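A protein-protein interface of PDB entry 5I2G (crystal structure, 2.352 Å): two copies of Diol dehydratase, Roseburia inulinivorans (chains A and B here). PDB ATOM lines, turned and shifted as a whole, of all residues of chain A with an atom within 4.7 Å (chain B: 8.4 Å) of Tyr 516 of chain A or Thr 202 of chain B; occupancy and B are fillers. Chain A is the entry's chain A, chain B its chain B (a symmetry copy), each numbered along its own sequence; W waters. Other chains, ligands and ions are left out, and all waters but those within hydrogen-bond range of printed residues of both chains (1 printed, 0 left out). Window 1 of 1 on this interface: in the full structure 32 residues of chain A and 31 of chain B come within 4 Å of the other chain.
CB of Pro 48 of chain B touches OH of Tyr 140 of chain A (3.4 Å).
Asn 512 of chain A touches Asp 197 of chain B.
CA of Ala 198 of chain B touches ND2 of Asn 512 of chain A (3.8 Å).
Ser 201 of chain B touches Ala 513 of chain A (OG to CA, 3.7 Å).
CA of Asp 199 of chain B touches OH of Tyr 516 of chain A (3.5 Å).
Ser 201 of chain B touches Tyr 516 of chain A (CB to CD2, 3.9 Å).
CG2 of Thr 202 of chain B touches CE1 of Tyr 516 of chain A, at 3.6 Å.
Ala 198 of chain B touches Pro 684 of chain A.
Of the 22 printed residues of chain B, 6 touch a printed residue of chain A.
Hydrophobic or aromatic side chains of chain B within 4 Å of the printed part of chain A: Pro 48.
Among the printed residues, 10 pairs touch across the chains.
Among the printed residues, no Asp or Glu carboxylate lies within 4 Å of a Lys or Arg side-chain nitrogen of the other chain.
Water W1 bridges the side-chain amide nitrogen (ND2) of Asn 512 of chain A and the backbone carbonyl oxygen (O) of Asp 197 of chain B.
O of Asp 199 of chain B sits at hydrogen-bond distance from OG1 of Thr 202 of chain B (3.2 Å).
No position is printed for both chains.
The side-chain hydroxyl (OH) of Tyr 516 of chain A sits at hydrogen-bond distance from the backbone carbonyl oxygen (O) of Ala 198 of chain B, at 2.7 Å.
The backbone carbonyl oxygen (O) of Tyr 140 of chain A sits at hydrogen-bond distance from the side-chain hydroxyl (OG) of Ser 201 of chain B (2.9 Å).
Of the printed residues of chain B, Tyr 140 of chain A touches Pro 48 and Ser 201.
Of the printed residues of chain B, Ala 513 of chain A touches Ser 201 (3.7 Å).
Asp 515 of chain A touches none of the printed residues of chain B.
Tyr 516 of chain A touches four residues of chain B.
No residue of chain B comes within 4 Å of Ala 517 of chain A.
Ala 519 of chain A touches none of the printed residues of chain B.
Of the printed residues of chain A, Asp 197 of chain B touches Asn 512.
Of the printed residues of chain A, Ala 198 of chain B touches Asn 512 (3.8 Å), Tyr 516 (2.7 Å) and Pro 684 (3.7 Å).
Printed residues of chain A within 4 Å of Ser 201 of chain B: Tyr 140, Ala 513 and Tyr 516.
The nearest residue of chain B that does not touch Tyr 516 of chain A is Tyr 200 of chain B (5.2 Å).
The nearest printed residue of chain B that does not touch Tyr 140 of chain A is Thr 202 of chain B (4.1 Å).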
ATOM      1  N   TYR A 140      16.831 -10.450  -3.032  1.00  0.00           N
ATOM      2  CA  TYR A 140      15.646 -11.285  -3.229  1.00  0.00           C
ATOM      3  C   TYR A 140      15.365 -12.195  -2.036  1.00  0.00           C
ATOM      4  O   TYR A 140      14.332 -12.862  -1.987  1.00  0.00           O
ATOM      5  CB  TYR A 140      15.791 -12.127  -4.506  1.00  0.00           C
ATOM      6  CG  TYR A 140      15.199 -11.499  -5.764  1.00  0.00           C
ATOM      7  CD1 TYR A 140      13.986 -10.792  -5.717  1.00  0.00           C
ATOM      8  CD2 TYR A 140      15.836 -11.619  -6.999  1.00  0.00           C
ATOM      9  CE1 TYR A 140      13.424 -10.240  -6.855  1.00  0.00           C
ATOM     10  CE2 TYR A 140      15.284 -11.048  -8.152  1.00  0.00           C
ATOM     11  CZ  TYR A 140      14.075 -10.362  -8.067  1.00  0.00           C
ATOM     12  OH  TYR A 140      13.515  -9.803  -9.195  1.00  0.00           O
ATOM     13  N   ASN A 512      16.015 -20.179  -4.007  1.00  0.00           N
ATOM     14  CA  ASN A 512      15.138 -19.587  -5.014  1.00  0.00           C
ATOM     15  C   ASN A 512      15.536 -18.170  -5.379  1.00  0.00           C
ATOM     16  O   ASN A 512      15.486 -17.808  -6.548  1.00  0.00           O
ATOM     17  CB  ASN A 512      13.678 -19.643  -4.561  1.00  0.00           C
ATOM     18  CG  ASN A 512      13.086 -21.047  -4.744  1.00  0.00           C
ATOM     19  OD1 ASN A 512      13.727 -21.916  -5.333  1.00  0.00           O
ATOM     20  ND2 ASN A 512      11.873 -21.261  -4.262  1.00  0.00           N
ATOM     21  N   ALA A 513      15.967 -17.385  -4.392  1.00  0.00           N
ATOM     22  CA  ALA A 513      16.487 -16.038  -4.635  1.00  0.00           C
ATOM     23  C   ALA A 513      17.683 -16.037  -5.586  1.00  0.00           C
ATOM     24  O   ALA A 513      17.751 -15.229  -6.513  1.00  0.00           O
ATOM     25  CB  ALA A 513      16.878 -15.369  -3.307  1.00  0.00           C
ATOM     26  N   ILE A 514      18.626 -16.946  -5.340  1.00  0.00           N
ATOM     27  CA  ILE A 514      19.810 -17.088  -6.176  1.00  0.00           C
ATOM     28  C   ILE A 514      19.466 -17.549  -7.596  1.00  0.00           C
ATOM     29  O   ILE A 514      20.054 -17.074  -8.571  1.00  0.00           O
ATOM     30  CB  ILE A 514      20.793 -18.079  -5.537  1.00  0.00           C
ATOM     31  CG1 ILE A 514      21.349 -17.485  -4.243  1.00  0.00           C
ATOM     32  CG2 ILE A 514      21.925 -18.396  -6.492  1.00  0.00           C
ATOM     33  CD1 ILE A 514      21.982 -18.487  -3.329  1.00  0.00           C
ATOM     34  N   ASP A 515      18.515 -18.477  -7.695  1.00  0.00           N
ATOM     35  CA  ASP A 515      17.979 -18.958  -8.970  1.00  0.00           C
ATOM     36  C   ASP A 515      17.454 -17.797  -9.838  1.00  0.00           C
ATOM     37  O   ASP A 515      17.814 -17.691 -11.015  1.00  0.00           O
ATOM     38  CB  ASP A 515      16.865 -19.974  -8.691  1.00  0.00           C
ATOM     39  CG  ASP A 515      16.744 -21.055  -9.756  1.00  0.00           C
ATOM     40  OD1 ASP A 515      17.193 -20.858 -10.898  1.00  0.00           O
ATOM     41  OD2 ASP A 515      16.184 -22.126  -9.441  1.00  0.00           O
ATOM     42  N   TYR A 516      16.622 -16.919  -9.265  1.00  0.00           N
ATOM     43  CA  TYR A 516      16.179 -15.727 -10.010  1.00  0.00           C
ATOM     44  C   TYR A 516      17.357 -14.854 -10.450  1.00  0.00           C
ATOM     45  O   TYR A 516      17.344 -14.291 -11.537  1.00  0.00           O
ATOM     46  CB  TYR A 516      15.189 -14.869  -9.194  1.00  0.00           C
ATOM     47  CG  TYR A 516      13.781 -15.413  -9.207  1.00  0.00           C
ATOM     48  CD1 TYR A 516      13.014 -15.396 -10.377  1.00  0.00           C
ATOM     49  CD2 TYR A 516      13.217 -15.948  -8.058  1.00  0.00           C
ATOM     50  CE1 TYR A 516      11.721 -15.918 -10.397  1.00  0.00           C
ATOM     51  CE2 TYR A 516      11.924 -16.462  -8.061  1.00  0.00           C
ATOM     52  CZ  TYR A 516      11.187 -16.456  -9.230  1.00  0.00           C
ATOM     53  OH  TYR A 516       9.914 -16.975  -9.212  1.00  0.00           O
ATOM     54  N   ALA A 517      18.384 -14.762  -9.621  1.00  0.00           N
ATOM     55  CA  ALA A 517      19.526 -13.922  -9.953  1.00  0.00           C
ATOM     56  C   ALA A 517      20.246 -14.444 -11.195  1.00  0.00           C
ATOM     57  O   ALA A 517      20.585 -13.664 -12.087  1.00  0.00           O
ATOM     58  CB  ALA A 517      20.492 -13.823  -8.759  1.00  0.00           C
ATOM     59  N   HIS A 518      20.472 -15.756 -11.268  1.00  0.00           N
ATOM     60  CA  HIS A 518      21.124 -16.329 -12.457  1.00  0.00           C
ATOM     61  C   HIS A 518      20.231 -16.256 -13.689  1.00  0.00           C
ATOM     62  O   HIS A 518      20.709 -15.974 -14.777  1.00  0.00           O
ATOM     63  CB  HIS A 518      21.548 -17.777 -12.225  1.00  0.00           C
ATOM     64  CG  HIS A 518      22.702 -17.898 -11.288  1.00  0.00           C
ATOM     65  ND1 HIS A 518      24.009 -17.780 -11.704  1.00  0.00           N
ATOM     66  CD2 HIS A 518      22.746 -18.078  -9.948  1.00  0.00           C
ATOM     67  CE1 HIS A 518      24.810 -17.884 -10.660  1.00  0.00           C
ATOM     68  NE2 HIS A 518      24.069 -18.070  -9.584  1.00  0.00           N
ATOM     69  N   ALA A 519      18.941 -16.508 -13.518  1.00  0.00           N
ATOM     70  CA  ALA A 519      18.002 -16.388 -14.629  1.00  0.00           C
ATOM     71  C   ALA A 519      18.024 -14.986 -15.207  1.00  0.00           C
ATOM     72  O   ALA A 519      17.956 -14.792 -16.417  1.00  0.00           O
ATOM     73  CB  ALA A 519      16.601 -16.734 -14.174  1.00  0.00           C
ATOM     74  N   LYS A 520      18.120 -13.994 -14.331  1.00  0.00           N
ATOM     75  CA  LYS A 520      17.989 -12.637 -14.786  1.00  0.00           C
ATOM     76  C   LYS A 520      19.319 -12.086 -15.294  1.00  0.00           C
ATOM     77  O   LYS A 520      19.360 -11.382 -16.309  1.00  0.00           O
ATOM     78  CB  LYS A 520      17.402 -11.777 -13.667  1.00  0.00           C
ATOM     79  CG  LYS A 520      15.897 -12.050 -13.452  1.00  0.00           C
ATOM     80  CD  LYS A 520      15.346 -11.363 -12.211  1.00  0.00           C
ATOM     81  CE  LYS A 520      13.811 -11.422 -12.132  1.00  0.00           C
ATOM     82  NZ  LYS A 520      13.191 -10.300 -12.889  1.00  0.00           N
ATOM     83  N   PRO A 684      12.065 -21.783  -9.349  1.00  0.00           N
ATOM     84  CA  PRO A 684      11.495 -20.942 -10.413  1.00  0.00           C
ATOM     85  C   PRO A 684      11.729 -21.485 -11.825  1.00  0.00           C
ATOM     86  O   PRO A 684      11.166 -20.928 -12.756  1.00  0.00           O
ATOM     87  CB  PRO A 684      12.223 -19.600 -10.242  1.00  0.00           C
ATOM     88  CG  PRO A 684      12.817 -19.633  -8.867  1.00  0.00           C
ATOM     89  CD  PRO A 684      13.111 -21.079  -8.582  1.00  0.00           C
ATOM     90  N   PRO B  48      16.317  -5.510  -7.380  1.00  0.00           N
ATOM     91  CA  PRO B  48      15.432  -5.814  -8.510  1.00  0.00           C
ATOM     92  C   PRO B  48      14.741  -4.559  -9.051  1.00  0.00           C
ATOM     93  O   PRO B  48      14.467  -3.604  -8.312  1.00  0.00           O
ATOM     94  CB  PRO B  48      14.426  -6.816  -7.928  1.00  0.00           C
ATOM     95  CG  PRO B  48      14.628  -6.811  -6.465  1.00  0.00           C
ATOM     96  CD  PRO B  48      15.918  -6.182  -6.132  1.00  0.00           C
ATOM     97  N   VAL B  50      11.817  -3.578 -10.082  1.00  0.00           N
ATOM     98  CA  VAL B  50      10.546  -3.044  -9.599  1.00  0.00           C
ATOM     99  C   VAL B  50      10.750  -2.343  -8.248  1.00  0.00           C
ATOM    100  O   VAL B  50      10.082  -1.346  -7.946  1.00  0.00           O
ATOM    101  CB  VAL B  50       9.446  -4.149  -9.497  1.00  0.00           C
ATOM    102  CG1 VAL B  50       9.797  -5.209  -8.438  1.00  0.00           C
ATOM    103  CG2 VAL B  50       8.102  -3.525  -9.206  1.00  0.00           C
ATOM    104  N   MET B  51      11.701  -2.837  -7.454  1.00  0.00           N
ATOM    105  CA  MET B  51      12.077  -2.153  -6.217  1.00  0.00           C
ATOM    106  C   MET B  51      12.776  -0.814  -6.521  1.00  0.00           C
ATOM    107  O   MET B  51      12.508   0.194  -5.867  1.00  0.00           O
ATOM    108  CB  MET B  51      12.980  -3.041  -5.364  1.00  0.00           C
ATOM    109  CG  MET B  51      13.444  -2.397  -4.078  1.00  0.00           C
ATOM    110  SD  MET B  51      12.064  -1.989  -2.996  1.00  0.00           S
ATOM    111  CE  MET B  51      11.357  -3.615  -2.715  1.00  0.00           C
ATOM    112  N   CYS B 193       1.624 -15.576   0.892  1.00  0.00           N
ATOM    113  CA  CYS B 193       2.929 -15.945   0.350  1.00  0.00           C
ATOM    114  C   CYS B 193       3.776 -16.608   1.410  1.00  0.00           C
ATOM    115  O   CYS B 193       3.941 -16.080   2.511  1.00  0.00           O
ATOM    116  CB  CYS B 193       3.659 -14.723  -0.210  1.00  0.00           C
ATOM    117  SG  CYS B 193       2.664 -13.734  -1.353  1.00  0.00           S
ATOM    118  N   ASP B 197       7.551 -20.736  -1.499  1.00  0.00           N
ATOM    119  CA  ASP B 197       6.850 -20.672  -2.788  1.00  0.00           C
ATOM    120  C   ASP B 197       7.851 -20.310  -3.871  1.00  0.00           C
ATOM    121  O   ASP B 197       8.743 -19.486  -3.637  1.00  0.00           O
ATOM    122  CB  ASP B 197       5.725 -19.636  -2.779  1.00  0.00           C
ATOM    123  CG  ASP B 197       4.642 -19.954  -1.776  1.00  0.00           C
ATOM    124  OD1 ASP B 197       4.558 -21.113  -1.334  1.00  0.00           O
ATOM    125  OD2 ASP B 197       3.853 -19.041  -1.443  1.00  0.00           O
ATOM    126  N   ALA B 198       7.699 -20.909  -5.049  1.00  0.00           N
ATOM    127  CA  ALA B 198       8.630 -20.675  -6.153  1.00  0.00           C
ATOM    128  C   ALA B 198       8.643 -19.209  -6.602  1.00  0.00           C
ATOM    129  O   ALA B 198       9.653 -18.724  -7.134  1.00  0.00           O
ATOM    130  CB  ALA B 198       8.299 -21.597  -7.342  1.00  0.00           C
ATOM    131  N   ASP B 199       7.538 -18.501  -6.367  1.00  0.00           N
ATOM    132  CA  ASP B 199       7.420 -17.103  -6.794  1.00  0.00           C
ATOM    133  C   ASP B 199       7.516 -16.112  -5.633  1.00  0.00           C
ATOM    134  O   ASP B 199       7.184 -14.938  -5.809  1.00  0.00           O
ATOM    135  CB  ASP B 199       6.094 -16.874  -7.542  1.00  0.00           C
ATOM    136  CG  ASP B 199       4.878 -16.989  -6.622  1.00  0.00           C
ATOM    137  OD1 ASP B 199       4.974 -17.654  -5.565  1.00  0.00           O
ATOM    138  OD2 ASP B 199       3.810 -16.424  -6.953  1.00  0.00           O
ATOM    139  N   TYR B 200       7.964 -16.566  -4.461  1.00  0.00           N
ATOM    140  CA  TYR B 200       8.000 -15.693  -3.281  1.00  0.00           C
ATOM    141  C   TYR B 200       8.872 -14.460  -3.519  1.00  0.00           C
ATOM    142  O   TYR B 200       8.411 -13.352  -3.292  1.00  0.00           O
ATOM    143  CB  TYR B 200       8.492 -16.448  -2.040  1.00  0.00           C
ATOM    144  CG  TYR B 200       8.472 -15.633  -0.765  1.00  0.00           C
ATOM    145  CD1 TYR B 200       7.336 -15.606   0.047  1.00  0.00           C
ATOM    146  CD2 TYR B 200       9.581 -14.883  -0.368  1.00  0.00           C
ATOM    147  CE1 TYR B 200       7.305 -14.860   1.224  1.00  0.00           C
ATOM    148  CE2 TYR B 200       9.560 -14.121   0.809  1.00  0.00           C
ATOM    149  CZ  TYR B 200       8.420 -14.121   1.601  1.00  0.00           C
ATOM    150  OH  TYR B 200       8.379 -13.379   2.762  1.00  0.00           O
ATOM    151  N   SER B 201      10.106 -14.643  -3.999  1.00  0.00           N
ATOM    152  CA  SER B 201      11.033 -13.515  -4.169  1.00  0.00           C
ATOM    153  C   SER B 201      10.454 -12.404  -5.047  1.00  0.00           C
ATOM    154  O   SER B 201      10.483 -11.244  -4.687  1.00  0.00           O
ATOM    155  CB  SER B 201      12.371 -13.968  -4.777  1.00  0.00           C
ATOM    156  OG  SER B 201      13.160 -14.720  -3.864  1.00  0.00           O
ATOM    157  N   THR B 202       9.941 -12.772  -6.206  1.00  0.00           N
ATOM    158  CA  THR B 202       9.433 -11.797  -7.155  1.00  0.00           C
ATOM    159  C   THR B 202       8.093 -11.216  -6.689  1.00  0.00           C
ATOM    160  O   THR B 202       7.879 -10.029  -6.782  1.00  0.00           O
ATOM    161  CB  THR B 202       9.286 -12.424  -8.549  1.00  0.00           C
ATOM    162  OG1 THR B 202       8.585 -13.671  -8.428  1.00  0.00           O
ATOM    163  CG2 THR B 202      10.672 -12.692  -9.149  1.00  0.00           C
ATOM    164  N   LYS B 203       7.208 -12.045  -6.155  1.00  0.00           N
ATOM    165  CA  LYS B 203       5.915 -11.560  -5.697  1.00  0.00           C
ATOM    166  C   LYS B 203       6.070 -10.622  -4.494  1.00  0.00           C
ATOM    167  O   LYS B 203       5.457  -9.555  -4.454  1.00  0.00           O
ATOM    168  CB  LYS B 203       4.983 -12.730  -5.351  1.00  0.00           C
ATOM    169  CG  LYS B 203       3.618 -12.295  -4.818  1.00  0.00           C
ATOM    170  CD  LYS B 203       2.562 -13.407  -4.909  1.00  0.00           C
ATOM    171  CE  LYS B 203       1.178 -12.833  -4.603  1.00  0.00           C
ATOM    172  NZ  LYS B 203       0.056 -13.809  -4.600  1.00  0.00           N
ATOM    173  N   MET B 204       6.894 -10.999  -3.522  1.00  0.00           N
ATOM    174  CA  MET B 204       7.066 -10.169  -2.331  1.00  0.00           C
ATOM    175  C   MET B 204       7.762  -8.859  -2.654  1.00  0.00           C
ATOM    176  O   MET B 204       7.367  -7.803  -2.159  1.00  0.00           O
ATOM    177  CB  MET B 204       7.849 -10.904  -1.243  1.00  0.00           C
ATOM    178  CG  MET B 204       7.022 -11.934  -0.503  1.00  0.00           C
ATOM    179  SD  MET B 204       5.676 -11.287   0.537  1.00  0.00           S
ATOM    180  CE  MET B 204       6.475  -9.913   1.374  1.00  0.00           C
ATOM    181  N   CYS B 205       8.801  -8.929  -3.480  1.00  0.00           N
ATOM    182  CA  CYS B 205       9.459  -7.720  -3.940  1.00  0.00           C
ATOM    183  C   CYS B 205       8.457  -6.789  -4.646  1.00  0.00           C
ATOM    184  O   CYS B 205       8.482  -5.572  -4.447  1.00  0.00           O
ATOM    185  CB  CYS B 205      10.615  -8.052  -4.879  1.00  0.00           C
ATOM    186  SG  CYS B 205      11.426  -6.558  -5.507  1.00  0.00           S
ATOM    187  N   PHE B 206       7.572  -7.360  -5.459  1.00  0.00           N
ATOM    188  CA  PHE B 206       6.577  -6.538  -6.127  1.00  0.00           C
ATOM    189  C   PHE B 206       5.610  -5.904  -5.113  1.00  0.00           C
ATOM    190  O   PHE B 206       5.283  -4.714  -5.192  1.00  0.00           O
ATOM    191  CB  PHE B 206       5.808  -7.350  -7.157  1.00  0.00           C
ATOM    192  CG  PHE B 206       4.687  -6.590  -7.786  1.00  0.00           C
ATOM    193  CD1 PHE B 206       4.948  -5.499  -8.603  1.00  0.00           C
ATOM    194  CD2 PHE B 206       3.370  -6.947  -7.548  1.00  0.00           C
ATOM    195  CE1 PHE B 206       3.914  -4.787  -9.172  1.00  0.00           C
ATOM    196  CE2 PHE B 206       2.330  -6.238  -8.123  1.00  0.00           C
ATOM    197  CZ  PHE B 206       2.600  -5.161  -8.930  1.00  0.00           C
ATOM    198  N   LEU B 207       5.177  -6.699  -4.145  1.00  0.00           N
ATOM    199  CA  LEU B 207       4.235  -6.216  -3.151  1.00  0.00           C
ATOM    200  C   LEU B 207       4.872  -5.211  -2.180  1.00  0.00           C
ATOM    201  O   LEU B 207       4.225  -4.250  -1.786  1.00  0.00           O
ATOM    202  CB  LEU B 207       3.622  -7.401  -2.391  1.00  0.00           C
ATOM    203  CG  LEU B 207       2.710  -8.322  -3.215  1.00  0.00           C
ATOM    204  CD1 LEU B 207       2.134  -9.423  -2.346  1.00  0.00           C
ATOM    205  CD2 LEU B 207       1.592  -7.522  -3.885  1.00  0.00           C
ATOM    206  N   GLU B 208       6.132  -5.417  -1.806  1.00  0.00           N
ATOM    207  CA  GLU B 208       6.847  -4.423  -1.001  1.00  0.00           C
ATOM    208  C   GLU B 208       6.955  -3.111  -1.757  1.00  0.00           C
ATOM    209  O   GLU B 208       6.932  -2.026  -1.163  1.00  0.00           O
ATOM    210  CB  GLU B 208       8.263  -4.892  -0.628  1.00  0.00           C
ATOM    211  CG  GLU B 208       8.323  -6.142   0.210  1.00  0.00           C
ATOM    212  CD  GLU B 208       8.000  -5.894   1.657  1.00  0.00           C
ATOM    213  OE1 GLU B 208       7.566  -4.766   1.984  1.00  0.00           O
ATOM    214  OE2 GLU B 208       8.196  -6.829   2.471  1.00  0.00           O
ATOM    215  N   SER B 209       7.113  -3.223  -3.069  1.00  0.00           N
ATOM    216  CA  SER B 209       7.279  -2.038  -3.903  1.00  0.00           C
ATOM    217  C   SER B 209       5.999  -1.231  -3.960  1.00  0.00           C
ATOM    218  O   SER B 209       6.042  -0.003  -4.041  1.00  0.00           O
ATOM    219  CB  SER B 209       7.731  -2.422  -5.312  1.00  0.00           C
ATOM    220  OG  SER B 209       8.980  -3.090  -5.249  1.00  0.00           O
ATOM    221  N   ARG B 537      -1.701 -11.594  -8.455  1.00  0.00           N
ATOM    222  CA  ARG B 537      -0.753 -12.342  -9.268  1.00  0.00           C
ATOM    223  C   ARG B 537       0.695 -12.059  -8.911  1.00  0.00           C
ATOM    224  O   ARG B 537       1.592 -12.774  -9.341  1.00  0.00           O
ATOM    225  CB  ARG B 537      -0.968 -12.043 -10.749  1.00  0.00           C
ATOM    226  CG  ARG B 537      -2.303 -12.495 -11.268  1.00  0.00           C
ATOM    227  CD  ARG B 537      -2.455 -12.139 -12.729  1.00  0.00           C
ATOM    228  NE  ARG B 537      -3.744 -12.577 -13.261  1.00  0.00           N
ATOM    229  CZ  ARG B 537      -4.160 -12.296 -14.491  1.00  0.00           C
ATOM    230  NH1 ARG B 537      -3.379 -11.585 -15.297  1.00  0.00           N
ATOM    231  NH2 ARG B 537      -5.341 -12.726 -14.920  1.00  0.00           N
ATOM    232  N   GLY B 538       0.923 -11.008  -8.138  1.00  0.00           N
ATOM    233  CA  GLY B 538       2.267 -10.663  -7.736  1.00  0.00           C
ATOM    234  C   GLY B 538       3.128 -10.144  -8.868  1.00  0.00           C
ATOM    235  O   GLY B 538       4.342 -10.293  -8.815  1.00  0.00           O
ATOM    236  N   MET B 539       2.515  -9.512  -9.875  1.00  0.00           N
ATOM    237  CA  MET B 539       3.272  -8.961 -11.005  1.00  0.00           C
ATOM    238  C   MET B 539       2.677  -7.672 -11.585  1.00  0.00           C
ATOM    239  O   MET B 539       1.453  -7.442 -11.539  1.00  0.00           O
ATOM    240  CB  MET B 539       3.380 -10.005 -12.108  1.00  0.00           C
ATOM    241  CG  MET B 539       2.060 -10.679 -12.374  1.00  0.00           C
ATOM    242  SD  MET B 539       2.279 -12.102 -13.433  1.00  0.00           S
ATOM    243  CE  MET B 539       3.131 -11.335 -14.800  1.00  0.00           C
ATOM    244  N   SER B 540       3.548  -6.837 -12.150  1.00  0.00           N
ATOM    245  CA  SER B 540       3.108  -5.541 -12.668  1.00  0.00           C
ATOM    246  C   SER B 540       2.251  -5.696 -13.925  1.00  0.00           C
ATOM    247  O   SER B 540       2.279  -6.743 -14.588  1.00  0.00           O
ATOM    248  CB  SER B 540       4.306  -4.637 -12.977  1.00  0.00           C
ATOM    249  OG  SER B 540       4.933  -5.039 -14.183  1.00  0.00           O
ATOM    250  N   GLU B 543       3.923  -6.541 -17.035  1.00  0.00           N
ATOM    251  CA  GLU B 543       4.366  -7.937 -17.177  1.00  0.00           C
ATOM    252  C   GLU B 543       3.247  -8.946 -17.367  1.00  0.00           C
ATOM    253  O   GLU B 543       3.523 -10.114 -17.554  1.00  0.00           O
ATOM    254  CB  GLU B 543       5.160  -8.395 -15.956  1.00  0.00           C
ATOM    255  CG  GLU B 543       6.278  -7.495 -15.518  1.00  0.00           C
ATOM    256  CD  GLU B 543       6.750  -7.853 -14.123  1.00  0.00           C
ATOM    257  OE1 GLU B 543       6.311  -7.200 -13.146  1.00  0.00           O
ATOM    258  OE2 GLU B 543       7.553  -8.804 -14.007  1.00  0.00           O
HETATM  259  O   HOH W   1      11.248 -19.311  -2.517  1.00  0.00           O
